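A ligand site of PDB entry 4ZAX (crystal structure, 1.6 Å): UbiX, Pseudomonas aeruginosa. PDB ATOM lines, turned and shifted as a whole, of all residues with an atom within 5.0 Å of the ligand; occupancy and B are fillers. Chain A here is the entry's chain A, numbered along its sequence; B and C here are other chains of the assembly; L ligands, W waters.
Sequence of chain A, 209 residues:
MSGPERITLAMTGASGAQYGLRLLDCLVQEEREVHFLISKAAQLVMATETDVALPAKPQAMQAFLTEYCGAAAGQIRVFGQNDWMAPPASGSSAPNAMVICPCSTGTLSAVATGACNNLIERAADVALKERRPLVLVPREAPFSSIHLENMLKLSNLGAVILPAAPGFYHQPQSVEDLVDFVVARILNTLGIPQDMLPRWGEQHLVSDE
The side-chain hydroxyl of Thr 107 lies within hydrogen-bond range of an oxygen (O8) of the ligand (2.4 Å). The side-chain hydroxyl of Ser 104 sits at hydrogen-bond distance from an oxygen (O8) of the ligand, at 2.5 Å. The side-chain hydroxyl (OG) of Ser 39 sits at hydrogen-bond distance from an oxygen (O7) of the ligand (2.6 Å). The backbone NH (N) of Gly 13 is in hydrogen-bond range of an oxygen (O7) of the ligand (2.7 Å). O of Gly 13 lies within hydrogen-bond range of O3 of the ligand, 2.6 Å away. O5 of the ligand is in hydrogen-bond range of O of Cys 116 of chain B (2.6 Å). O of Arg 139 is in hydrogen-bond range of N1 of the ligand (3.0 Å). The guanidinium group (NH2) of Arg 139 is in hydrogen-bond range of an oxygen (O2) of the ligand (2.8 Å). The backbone NH (N) of Thr 105 sits at hydrogen-bond distance from an oxygen (O1) of the ligand (2.8 Å). An oxygen (O2) of the ligand lies within hydrogen-bond range of the backbone NH (N) of Ser 15, 2.9 Å away.
N of Thr 107 lies within hydrogen-bond range of OG of Ser 104. The backbone NH (N) of Ser 104 is in hydrogen-bond range of the side-chain hydroxyl (OG1) of Thr 12 (2.8 Å). The side-chain hydroxyl (OG) of Ser 104 sits close to the backbone NH (N) of Gly 106 (3.5 Å). N of Ala 42 lies within hydrogen-bond range of OG of Ser 39. The side-chain hydroxyl (OG1) of Thr 105 sits at hydrogen-bond distance from the guanidinium group (NH1) of Arg 122 of chain B, 3.4 Å away. NE1 of Trp 200 of chain C lies within hydrogen-bond range of O of Trp 84 of chain B (3.0 Å). The backbone NH of Tyr 169 of chain C sits at hydrogen-bond distance from the side-chain carboxylate of Glu 49 (3.4 Å). OG1 of Thr 48 sits at hydrogen-bond distance from O of Leu 44, at 2.9 Å.
Thr 12 touches the ligand (CB to O7, 3.4 Å). Ala 14 touches the ligand (CA to C10, 3.3 Å). CB of Ala 41 touches O3 of the ligand, at 3.5 Å. CD1 of Leu 44 touches C16 of the ligand, at 3.8 Å. Val 45 touches the ligand. Glu 49 touches the ligand. Glu 140 touches the ligand. Trp 84 of chain B touches the ligand. NH2 of Arg 122 of chain B touches C4 of the ligand, at 3.7 Å. Tyr 169 of chain C touches the ligand. CH2 of Trp 200 of chain C touches C13 of the ligand, 3.4 Å away. Hydrophobic or aromatic side chains that line the ligand: Ala 14, Ala 41, Leu 44, Val 45, Trp 84 of chain B, Tyr 169 of chain C and Trp 200 of chain C. Along chain A the residues within 4 Å of the ligand span positions 12 to 140.
Water W1 lies within hydrogen-bond range of an oxygen (O5) of the ligand (2.5 Å) and the backbone carbonyl oxygen (O) of Asn 117 of chain B (3.4 Å). Water W4 lies within hydrogen-bond range of an oxygen (O4) of the ligand (2.8 Å), the side-chain hydroxyl of Thr 105 (2.9 Å) and the backbone NH of Gly 106 (3.2 Å). Water W7 lies within hydrogen-bond range of the backbone carbonyl oxygen (O) of Cys 103 (2.7 Å), the backbone NH (N) of Arg 139 (2.8 Å) and an oxygen (O1) of the ligand (3.1 Å). Water W3 lies within hydrogen-bond range of the backbone NH of Ala 41 (2.9 Å) and an oxygen (O9) of the ligand (3.2 Å).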
ATOM      1  N   THR A  12     -14.920   4.899   6.408  1.00  0.00           N
ATOM      2  CA  THR A  12     -13.994   3.794   6.630  1.00  0.00           C
ATOM      3  C   THR A  12     -13.981   3.389   8.126  1.00  0.00           C
ATOM      4  O   THR A  12     -14.606   4.039   8.960  1.00  0.00           O
ATOM      5  CB  THR A  12     -12.557   4.058   6.069  1.00  0.00           C
ATOM      6  OG1 THR A  12     -11.944   5.149   6.788  1.00  0.00           O
ATOM      7  CG2 THR A  12     -12.623   4.436   4.641  1.00  0.00           C
ATOM      8  N   GLY A  13     -13.240   2.379   8.391  1.00  0.00           N
ATOM      9  CA  GLY A  13     -13.354   1.634   9.624  1.00  0.00           C
ATOM     10  C   GLY A  13     -12.768   2.195  10.909  1.00  0.00           C
ATOM     11  O   GLY A  13     -12.106   1.471  11.579  1.00  0.00           O
ATOM     12  N   ALA A  14     -12.937   3.479  11.181  1.00  0.00           N
ATOM     13  CA  ALA A  14     -12.541   4.045  12.450  1.00  0.00           C
ATOM     14  C   ALA A  14     -13.890   4.211  13.229  1.00  0.00           C
ATOM     15  O   ALA A  14     -14.972   4.387  12.645  1.00  0.00           O
ATOM     16  CB  ALA A  14     -11.904   5.360  12.280  1.00  0.00           C
ATOM     17  N   SER A  15     -13.761   4.250  14.534  1.00  0.00           N
ATOM     18  CA  SER A  15     -14.877   4.721  15.389  1.00  0.00           C
ATOM     19  C   SER A  15     -15.326   6.056  15.016  1.00  0.00           C
ATOM     20  O   SER A  15     -14.553   6.965  14.539  1.00  0.00           O
ATOM     21  CB  SER A  15     -14.475   4.593  16.850  1.00  0.00           C
ATOM     22  OG  SER A  15     -15.603   4.840  17.645  1.00  0.00           O
ATOM     23  N   SER A  39     -16.644   1.172   3.494  1.00  0.00           N
ATOM     24  CA  SER A  39     -15.829  -0.010   3.503  1.00  0.00           C
ATOM     25  C   SER A  39     -16.526  -1.121   4.340  1.00  0.00           C
ATOM     26  O   SER A  39     -17.428  -0.846   5.136  1.00  0.00           O
ATOM     27  CB  SER A  39     -14.448   0.285   4.070  1.00  0.00           C
ATOM     28  OG  SER A  39     -14.521   0.468   5.473  1.00  0.00           O
ATOM     29  N   ALA A  41     -15.115  -2.801   6.778  1.00  0.00           N
ATOM     30  CA  ALA A  41     -14.866  -2.516   8.196  1.00  0.00           C
ATOM     31  C   ALA A  41     -15.785  -1.394   8.750  1.00  0.00           C
ATOM     32  O   ALA A  41     -16.264  -1.492   9.841  1.00  0.00           O
ATOM     33  CB  ALA A  41     -13.402  -2.206   8.451  1.00  0.00           C
ATOM     34  N   ALA A  42     -16.112  -0.370   7.965  1.00  0.00           N
ATOM     35  CA  ALA A  42     -16.971   0.686   8.374  1.00  0.00           C
ATOM     36  C   ALA A  42     -18.397   0.130   8.613  1.00  0.00           C
ATOM     37  O   ALA A  42     -19.092   0.650   9.455  1.00  0.00           O
ATOM     38  CB  ALA A  42     -17.045   1.847   7.415  1.00  0.00           C
ATOM     39  N   LEU A  44     -19.060  -2.771   9.714  1.00  0.00           N
ATOM     40  CA  LEU A  44     -18.997  -3.461  11.027  1.00  0.00           C
ATOM     41  C   LEU A  44     -18.941  -2.434  12.122  1.00  0.00           C
ATOM     42  O   LEU A  44     -19.569  -2.581  13.141  1.00  0.00           O
ATOM     43  CB  LEU A  44     -17.786  -4.389  11.118  1.00  0.00           C
ATOM     44  CG  LEU A  44     -17.811  -5.707  11.921  1.00  0.00           C
ATOM     45  CD1 LEU A  44     -16.380  -5.947  12.346  1.00  0.00           C
ATOM     46  CD2 LEU A  44     -18.744  -5.774  13.118  1.00  0.00           C
ATOM     47  N   VAL A  45     -18.222  -1.323  11.941  1.00  0.00           N
ATOM     48  CA  VAL A  45     -18.322  -0.258  12.938  1.00  0.00           C
ATOM     49  C   VAL A  45     -19.761   0.277  13.133  1.00  0.00           C
ATOM     50  O   VAL A  45     -20.201   0.502  14.237  1.00  0.00           O
ATOM     51  CB  VAL A  45     -17.380   0.948  12.608  1.00  0.00           C
ATOM     52  CG1 VAL A  45     -17.581   2.085  13.550  1.00  0.00           C
ATOM     53  CG2 VAL A  45     -15.955   0.484  12.624  1.00  0.00           C
ATOM     54  N   THR A  48     -21.721  -2.161  15.175  1.00  0.00           N
ATOM     55  CA  THR A  48     -21.206  -2.151  16.581  1.00  0.00           C
ATOM     56  C   THR A  48     -21.646  -0.905  17.362  1.00  0.00           C
ATOM     57  O   THR A  48     -22.076  -1.024  18.477  1.00  0.00           O
ATOM     58  CB  THR A  48     -19.643  -2.264  16.587  1.00  0.00           C
ATOM     59  OG1 THR A  48     -19.187  -3.397  15.866  1.00  0.00           O
ATOM     60  CG2 THR A  48     -19.062  -2.391  17.977  1.00  0.00           C
ATOM     61  N   GLU A  49     -21.636   0.304  16.797  1.00  0.00           N
ATOM     62  CA  GLU A  49     -21.739   1.559  17.570  1.00  0.00           C
ATOM     63  C   GLU A  49     -23.015   2.203  17.402  1.00  0.00           C
ATOM     64  O   GLU A  49     -23.219   3.168  18.027  1.00  0.00           O
ATOM     65  CB  GLU A  49     -20.771   2.704  17.009  1.00  0.00           C
ATOM     66  CG  GLU A  49     -19.430   2.280  16.957  1.00  0.00           C
ATOM     67  CD  GLU A  49     -18.465   3.471  16.710  1.00  0.00           C
ATOM     68  OE1 GLU A  49     -18.717   4.543  16.048  1.00  0.00           O
ATOM     69  OE2 GLU A  49     -17.478   3.214  17.303  1.00  0.00           O
ATOM     70  N   CYS A 103     -12.018   8.453   8.900  1.00  0.00           N
ATOM     71  CA  CYS A 103     -10.912   7.939   8.105  1.00  0.00           C
ATOM     72  C   CYS A 103     -10.043   7.050   9.001  1.00  0.00           C
ATOM     73  O   CYS A 103      -9.385   7.584   9.909  1.00  0.00           O
ATOM     74  CB  CYS A 103     -10.088   9.086   7.677  1.00  0.00           C
ATOM     75  SG  CYS A 103      -8.723   8.601   6.521  1.00  0.00           S
ATOM     76  N   SER A 104     -10.037   5.779   8.743  1.00  0.00           N
ATOM     77  CA  SER A 104      -9.178   4.856   9.490  1.00  0.00           C
ATOM     78  C   SER A 104      -7.692   5.177   9.259  1.00  0.00           C
ATOM     79  O   SER A 104      -7.294   5.797   8.248  1.00  0.00           O
ATOM     80  CB  SER A 104      -9.379   3.413   9.067  1.00  0.00           C
ATOM     81  OG  SER A 104      -8.986   3.225   7.772  1.00  0.00           O
ATOM     82  N   THR A 105      -6.828   4.729  10.178  1.00  0.00           N
ATOM     83  CA  THR A 105      -5.409   4.945   9.982  1.00  0.00           C
ATOM     84  C   THR A 105      -4.956   4.143   8.753  1.00  0.00           C
ATOM     85  O   THR A 105      -4.069   4.587   8.006  1.00  0.00           O
ATOM     86  CB  THR A 105      -4.578   4.565  11.248  1.00  0.00           C
ATOM     87  OG1 THR A 105      -4.713   3.185  11.524  1.00  0.00           O
ATOM     88  CG2 THR A 105      -5.012   5.394  12.368  1.00  0.00           C
ATOM     89  N   GLY A 106      -5.572   2.999   8.426  1.00  0.00           N
ATOM     90  CA  GLY A 106      -5.244   2.212   7.261  1.00  0.00           C
ATOM     91  C   GLY A 106      -5.585   2.973   5.965  1.00  0.00           C
ATOM     92  O   GLY A 106      -4.850   2.996   4.985  1.00  0.00           O
ATOM     93  N   THR A 107      -6.723   3.687   5.951  1.00  0.00           N
ATOM     94  CA  THR A 107      -7.073   4.490   4.811  1.00  0.00           C
ATOM     95  C   THR A 107      -6.159   5.683   4.682  1.00  0.00           C
ATOM     96  O   THR A 107      -5.677   6.055   3.577  1.00  0.00           O
ATOM     97  CB  THR A 107      -8.555   4.889   4.873  1.00  0.00           C
ATOM     98  OG1 THR A 107      -9.342   3.690   4.730  1.00  0.00           O
ATOM     99  CG2 THR A 107      -8.877   5.807   3.729  1.00  0.00           C
ATOM    100  N   ASN A 118      -8.902  -0.114  -3.428  1.00  0.00           N
ATOM    101  CA  ASN A 118     -10.354  -0.139  -3.555  1.00  0.00           C
ATOM    102  C   ASN A 118     -10.820   1.229  -4.042  1.00  0.00           C
ATOM    103  O   ASN A 118     -10.008   2.165  -4.234  1.00  0.00           O
ATOM    104  CB  ASN A 118     -10.974  -0.464  -2.238  1.00  0.00           C
ATOM    105  CG  ASN A 118     -10.527   0.462  -1.120  1.00  0.00           C
ATOM    106  OD1 ASN A 118     -10.658   1.663  -1.228  1.00  0.00           O
ATOM    107  ND2 ASN A 118      -9.973  -0.103  -0.047  1.00  0.00           N
ATOM    108  N   ARG A 139      -9.923   9.339  13.405  1.00  0.00           N
ATOM    109  CA  ARG A 139     -10.353   9.158  14.856  1.00  0.00           C
ATOM    110  C   ARG A 139      -9.525   8.035  15.444  1.00  0.00           C
ATOM    111  O   ARG A 139      -9.692   6.876  15.126  1.00  0.00           O
ATOM    112  CB  ARG A 139     -11.850   8.769  14.912  1.00  0.00           C
ATOM    113  CG  ARG A 139     -12.528   8.958  16.310  1.00  0.00           C
ATOM    114  CD  ARG A 139     -11.776   8.473  17.548  1.00  0.00           C
ATOM    115  NE  ARG A 139     -11.521   7.107  17.536  1.00  0.00           N
ATOM    116  CZ  ARG A 139     -10.754   6.525  18.454  1.00  0.00           C
ATOM    117  NH1 ARG A 139     -10.255   7.181  19.500  1.00  0.00           N
ATOM    118  NH2 ARG A 139     -10.474   5.281  18.287  1.00  0.00           N
ATOM    119  N   GLU A 140      -8.463   8.443  16.143  1.00  0.00           N
ATOM    120  CA  GLU A 140      -7.497   7.469  16.661  1.00  0.00           C
ATOM    121  C   GLU A 140      -6.871   8.189  17.821  1.00  0.00           C
ATOM    122  O   GLU A 140      -6.767   9.420  17.857  1.00  0.00           O
ATOM    123  CB  GLU A 140      -6.466   7.087  15.589  1.00  0.00           C
ATOM    124  CG  GLU A 140      -5.467   6.051  16.080  1.00  0.00           C
ATOM    125  CD  GLU A 140      -6.111   4.815  16.582  1.00  0.00           C
ATOM    126  OE1 GLU A 140      -6.510   4.795  17.786  1.00  0.00           O
ATOM    127  OE2 GLU A 140      -6.250   3.839  15.761  1.00  0.00           O
ATOM    128  N   TRP B  84     -11.810  -8.224  14.064  1.00  0.00           N
ATOM    129  CA  TRP B  84     -11.648  -6.951  14.741  1.00  0.00           C
ATOM    130  C   TRP B  84     -12.159  -6.939  16.181  1.00  0.00           C
ATOM    131  O   TRP B  84     -11.860  -5.979  16.899  1.00  0.00           O
ATOM    132  CB  TRP B  84     -12.305  -5.776  13.947  1.00  0.00           C
ATOM    133  CG  TRP B  84     -11.860  -5.815  12.444  1.00  0.00           C
ATOM    134  CD1 TRP B  84     -12.675  -6.063  11.328  1.00  0.00           C
ATOM    135  CD2 TRP B  84     -10.526  -5.660  11.915  1.00  0.00           C
ATOM    136  NE1 TRP B  84     -11.915  -6.068  10.203  1.00  0.00           N
ATOM    137  CE2 TRP B  84     -10.616  -5.802  10.508  1.00  0.00           C
ATOM    138  CE3 TRP B  84      -9.251  -5.417  12.491  1.00  0.00           C
ATOM    139  CZ2 TRP B  84      -9.485  -5.737   9.679  1.00  0.00           C
ATOM    140  CZ3 TRP B  84      -8.164  -5.288  11.648  1.00  0.00           C
ATOM    141  CH2 TRP B  84      -8.291  -5.494  10.252  1.00  0.00           C
ATOM    142  N   MET B  85     -12.872  -7.962  16.593  1.00  0.00           N
ATOM    143  CA  MET B  85     -13.261  -8.156  17.991  1.00  0.00           C
ATOM    144  C   MET B  85     -12.162  -8.702  18.876  1.00  0.00           C
ATOM    145  O   MET B  85     -12.330  -8.724  20.086  1.00  0.00           O
ATOM    146  CB  MET B  85     -14.541  -9.057  18.054  1.00  0.00           C
ATOM    147  CG  MET B  85     -15.671  -8.472  17.178  1.00  0.00           C
ATOM    148  SD  MET B  85     -16.033  -6.663  17.174  1.00  0.00           S
ATOM    149  CE  MET B  85     -16.098  -6.234  15.413  1.00  0.00           C
ATOM    150  N   CYS B 116      -2.301  -1.447   7.764  1.00  0.00           N
ATOM    151  CA  CYS B 116      -3.573  -2.089   8.389  1.00  0.00           C
ATOM    152  C   CYS B 116      -4.567  -2.869   7.470  1.00  0.00           C
ATOM    153  O   CYS B 116      -5.769  -2.758   7.631  1.00  0.00           O
ATOM    154  CB  CYS B 116      -4.351  -1.043   9.137  1.00  0.00           C
ATOM    155  SG  CYS B 116      -3.487  -0.219  10.518  1.00  0.00           S
ATOM    156  N   ASN B 117      -4.144  -3.823   6.681  1.00  0.00           N
ATOM    157  CA  ASN B 117      -4.974  -4.481   5.696  1.00  0.00           C
ATOM    158  C   ASN B 117      -5.657  -5.728   6.359  1.00  0.00           C
ATOM    159  O   ASN B 117      -6.533  -6.344   5.756  1.00  0.00           O
ATOM    160  CB  ASN B 117      -4.099  -5.062   4.508  1.00  0.00           C
ATOM    161  CG  ASN B 117      -3.248  -3.992   3.679  1.00  0.00           C
ATOM    162  OD1 ASN B 117      -3.865  -3.077   3.025  1.00  0.00           O
ATOM    163  ND2 ASN B 117      -1.804  -4.132   3.673  1.00  0.00           N
ATOM    164  N   ASN B 118      -5.157  -6.155   7.511  1.00  0.00           N
ATOM    165  CA  ASN B 118      -5.620  -7.349   8.208  1.00  0.00           C
ATOM    166  C   ASN B 118      -5.265  -7.216   9.684  1.00  0.00           C
ATOM    167  O   ASN B 118      -4.642  -6.218  10.118  1.00  0.00           O
ATOM    168  CB  ASN B 118      -4.974  -8.561   7.622  1.00  0.00           C
ATOM    169  CG  ASN B 118      -3.457  -8.480   7.599  1.00  0.00           C
ATOM    170  OD1 ASN B 118      -2.839  -8.270   8.620  1.00  0.00           O
ATOM    171  ND2 ASN B 118      -2.859  -8.625   6.417  1.00  0.00           N
ATOM    172  N   ARG B 122      -2.854  -4.434  11.645  1.00  0.00           N
ATOM    173  CA  ARG B 122      -3.479  -3.551  12.602  1.00  0.00           C
ATOM    174  C   ARG B 122      -2.892  -3.737  14.001  1.00  0.00           C
ATOM    175  O   ARG B 122      -2.658  -2.750  14.746  1.00  0.00           O
ATOM    176  CB  ARG B 122      -5.002  -3.734  12.627  1.00  0.00           C
ATOM    177  CG  ARG B 122      -5.704  -2.917  13.753  1.00  0.00           C
ATOM    178  CD  ARG B 122      -5.537  -1.411  13.674  1.00  0.00           C
ATOM    179  NE  ARG B 122      -6.349  -0.795  14.706  1.00  0.00           N
ATOM    180  CZ  ARG B 122      -6.312   0.529  14.942  1.00  0.00           C
ATOM    181  NH1 ARG B 122      -5.523   1.330  14.273  1.00  0.00           N
ATOM    182  NH2 ARG B 122      -7.079   1.007  15.899  1.00  0.00           N
ATOM    183  N   TYR C 169     -17.215   3.386  20.730  1.00  0.00           N
ATOM    184  CA  TYR C 169     -17.426   1.965  20.733  1.00  0.00           C
ATOM    185  C   TYR C 169     -17.789   1.425  22.111  1.00  0.00           C
ATOM    186  O   TYR C 169     -18.022   0.248  22.199  1.00  0.00           O
ATOM    187  CB  TYR C 169     -16.317   1.200  20.095  1.00  0.00           C
ATOM    188  CG  TYR C 169     -14.900   1.456  20.639  1.00  0.00           C
ATOM    189  CD1 TYR C 169     -14.383   0.756  21.656  1.00  0.00           C
ATOM    190  CD2 TYR C 169     -14.078   2.414  20.045  1.00  0.00           C
ATOM    191  CE1 TYR C 169     -13.090   0.932  22.111  1.00  0.00           C
ATOM    192  CE2 TYR C 169     -12.775   2.612  20.501  1.00  0.00           C
ATOM    193  CZ  TYR C 169     -12.270   1.852  21.468  1.00  0.00           C
ATOM    194  OH  TYR C 169     -10.992   2.036  21.917  1.00  0.00           O
ATOM    195  N   TRP C 200     -10.545  -4.214  25.503  1.00  0.00           N
ATOM    196  CA  TRP C 200     -11.100  -4.749  24.300  1.00  0.00           C
ATOM    197  C   TRP C 200     -10.810  -6.201  24.092  1.00  0.00           C
ATOM    198  O   TRP C 200      -9.657  -6.665  24.067  1.00  0.00           O
ATOM    199  CB  TRP C 200     -10.585  -3.983  23.012  1.00  0.00           C
ATOM    200  CG  TRP C 200     -11.264  -4.354  21.781  1.00  0.00           C
ATOM    201  CD1 TRP C 200     -10.745  -5.051  20.725  1.00  0.00           C
ATOM    202  CD2 TRP C 200     -12.548  -3.970  21.385  1.00  0.00           C
ATOM    203  NE1 TRP C 200     -11.657  -5.197  19.753  1.00  0.00           N
ATOM    204  CE2 TRP C 200     -12.783  -4.516  20.120  1.00  0.00           C
ATOM    205  CE3 TRP C 200     -13.600  -3.270  22.019  1.00  0.00           C
ATOM    206  CZ2 TRP C 200     -13.997  -4.388  19.454  1.00  0.00           C
ATOM    207  CZ3 TRP C 200     -14.772  -3.108  21.348  1.00  0.00           C
ATOM    208  CH2 TRP C 200     -15.015  -3.702  20.108  1.00  0.00           C
HETATM  209  C1  LIG L   1     -12.059  -1.685  13.178  1.00  0.00           C
HETATM  210  C2  LIG L   1     -13.284  -2.202  13.648  1.00  0.00           C
HETATM  211  C3  LIG L   1     -13.887  -1.725  14.806  1.00  0.00           C
HETATM  212  C4  LIG L   1     -10.031   1.308  13.742  1.00  0.00           C
HETATM  213  C5  LIG L   1     -13.254  -0.678  15.559  1.00  0.00           C
HETATM  214  N1  LIG L   1      -9.572   3.964  14.297  1.00  0.00           N
HETATM  215  C6  LIG L   1      -8.878   3.325  13.275  1.00  0.00           C
HETATM  216  C7  LIG L   1     -14.881   0.891  16.608  1.00  0.00           C
HETATM  217  C8  LIG L   1     -13.770  -0.102  16.823  1.00  0.00           C
HETATM  218  C9  LIG L   1     -11.820   1.473  16.963  1.00  0.00           C
HETATM  219  O1  LIG L   1      -8.051   4.073  12.632  1.00  0.00           O
HETATM  220  N2  LIG L   1      -9.135   2.046  12.973  1.00  0.00           N
HETATM  221  C10 LIG L   1     -10.627   3.345  15.033  1.00  0.00           C
HETATM  222  O2  LIG L   1     -11.205   4.091  15.856  1.00  0.00           O
HETATM  223  C11 LIG L   1     -10.616   1.910  14.900  1.00  0.00           C
HETATM  224  N3  LIG L   1     -11.489   0.997  15.637  1.00  0.00           N
HETATM  225  C12 LIG L   1     -12.616   0.359  17.657  1.00  0.00           C
HETATM  226  C13 LIG L   1     -14.297  -1.326  17.779  1.00  0.00           C
HETATM  227  C14 LIG L   1     -12.051  -0.110  15.032  1.00  0.00           C
HETATM  228  C15 LIG L   1     -15.303  -2.157  15.117  1.00  0.00           C
HETATM  229  C16 LIG L   1     -14.011  -3.027  12.758  1.00  0.00           C
HETATM  230  C17 LIG L   1     -11.399  -0.643  13.940  1.00  0.00           C
HETATM  231  N4  LIG L   1     -10.279   0.001  13.453  1.00  0.00           N
HETATM  232  C18 LIG L   1      -9.354  -0.756  12.472  1.00  0.00           C
HETATM  233  C19 LIG L   1      -9.684  -0.519  11.007  1.00  0.00           C
HETATM  234  O3  LIG L   1     -11.091  -0.811  10.753  1.00  0.00           O
HETATM  235  C20 LIG L   1      -8.765  -1.367  10.176  1.00  0.00           C
HETATM  236  O4  LIG L   1      -7.402  -1.285  10.418  1.00  0.00           O
HETATM  237  C21 LIG L   1      -9.306  -1.756   8.842  1.00  0.00           C
HETATM  238  O5  LIG L   1      -8.371  -2.643   8.080  1.00  0.00           O
HETATM  239  C22 LIG L   1      -9.589  -0.427   8.164  1.00  0.00           C
HETATM  240  O6  LIG L   1     -10.038  -0.781   6.854  1.00  0.00           O
HETATM  241  P1  LIG L   1     -10.817   0.387   5.978  1.00  0.00           P
HETATM  242  O7  LIG L   1     -12.163   0.722   6.523  1.00  0.00           O
HETATM  243  O8  LIG L   1      -9.719   1.619   5.962  1.00  0.00           O
HETATM  244  O9  LIG L   1     -10.949  -0.216   4.520  1.00  0.00           O
HETATM  245  O   HOH W   1      -9.124  -4.272   6.400  1.00  0.00           O
HETATM  246  O   HOH W   2      -7.208  -0.095   5.387  1.00  0.00           O
HETATM  247  O   HOH W   3     -12.794  -2.722   5.077  1.00  0.00           O
HETATM  248  O   HOH W   4      -6.982   1.483  10.866  1.00  0.00           O
HETATM  249  O   HOH W   5      -9.145  -1.741   3.276  1.00  0.00           O
HETATM  250  O   HOH W   6      -9.165  -0.301  16.820  1.00  0.00           O
HETATM  251  O   HOH W   7      -8.380   7.181  12.366  1.00  0.00           O
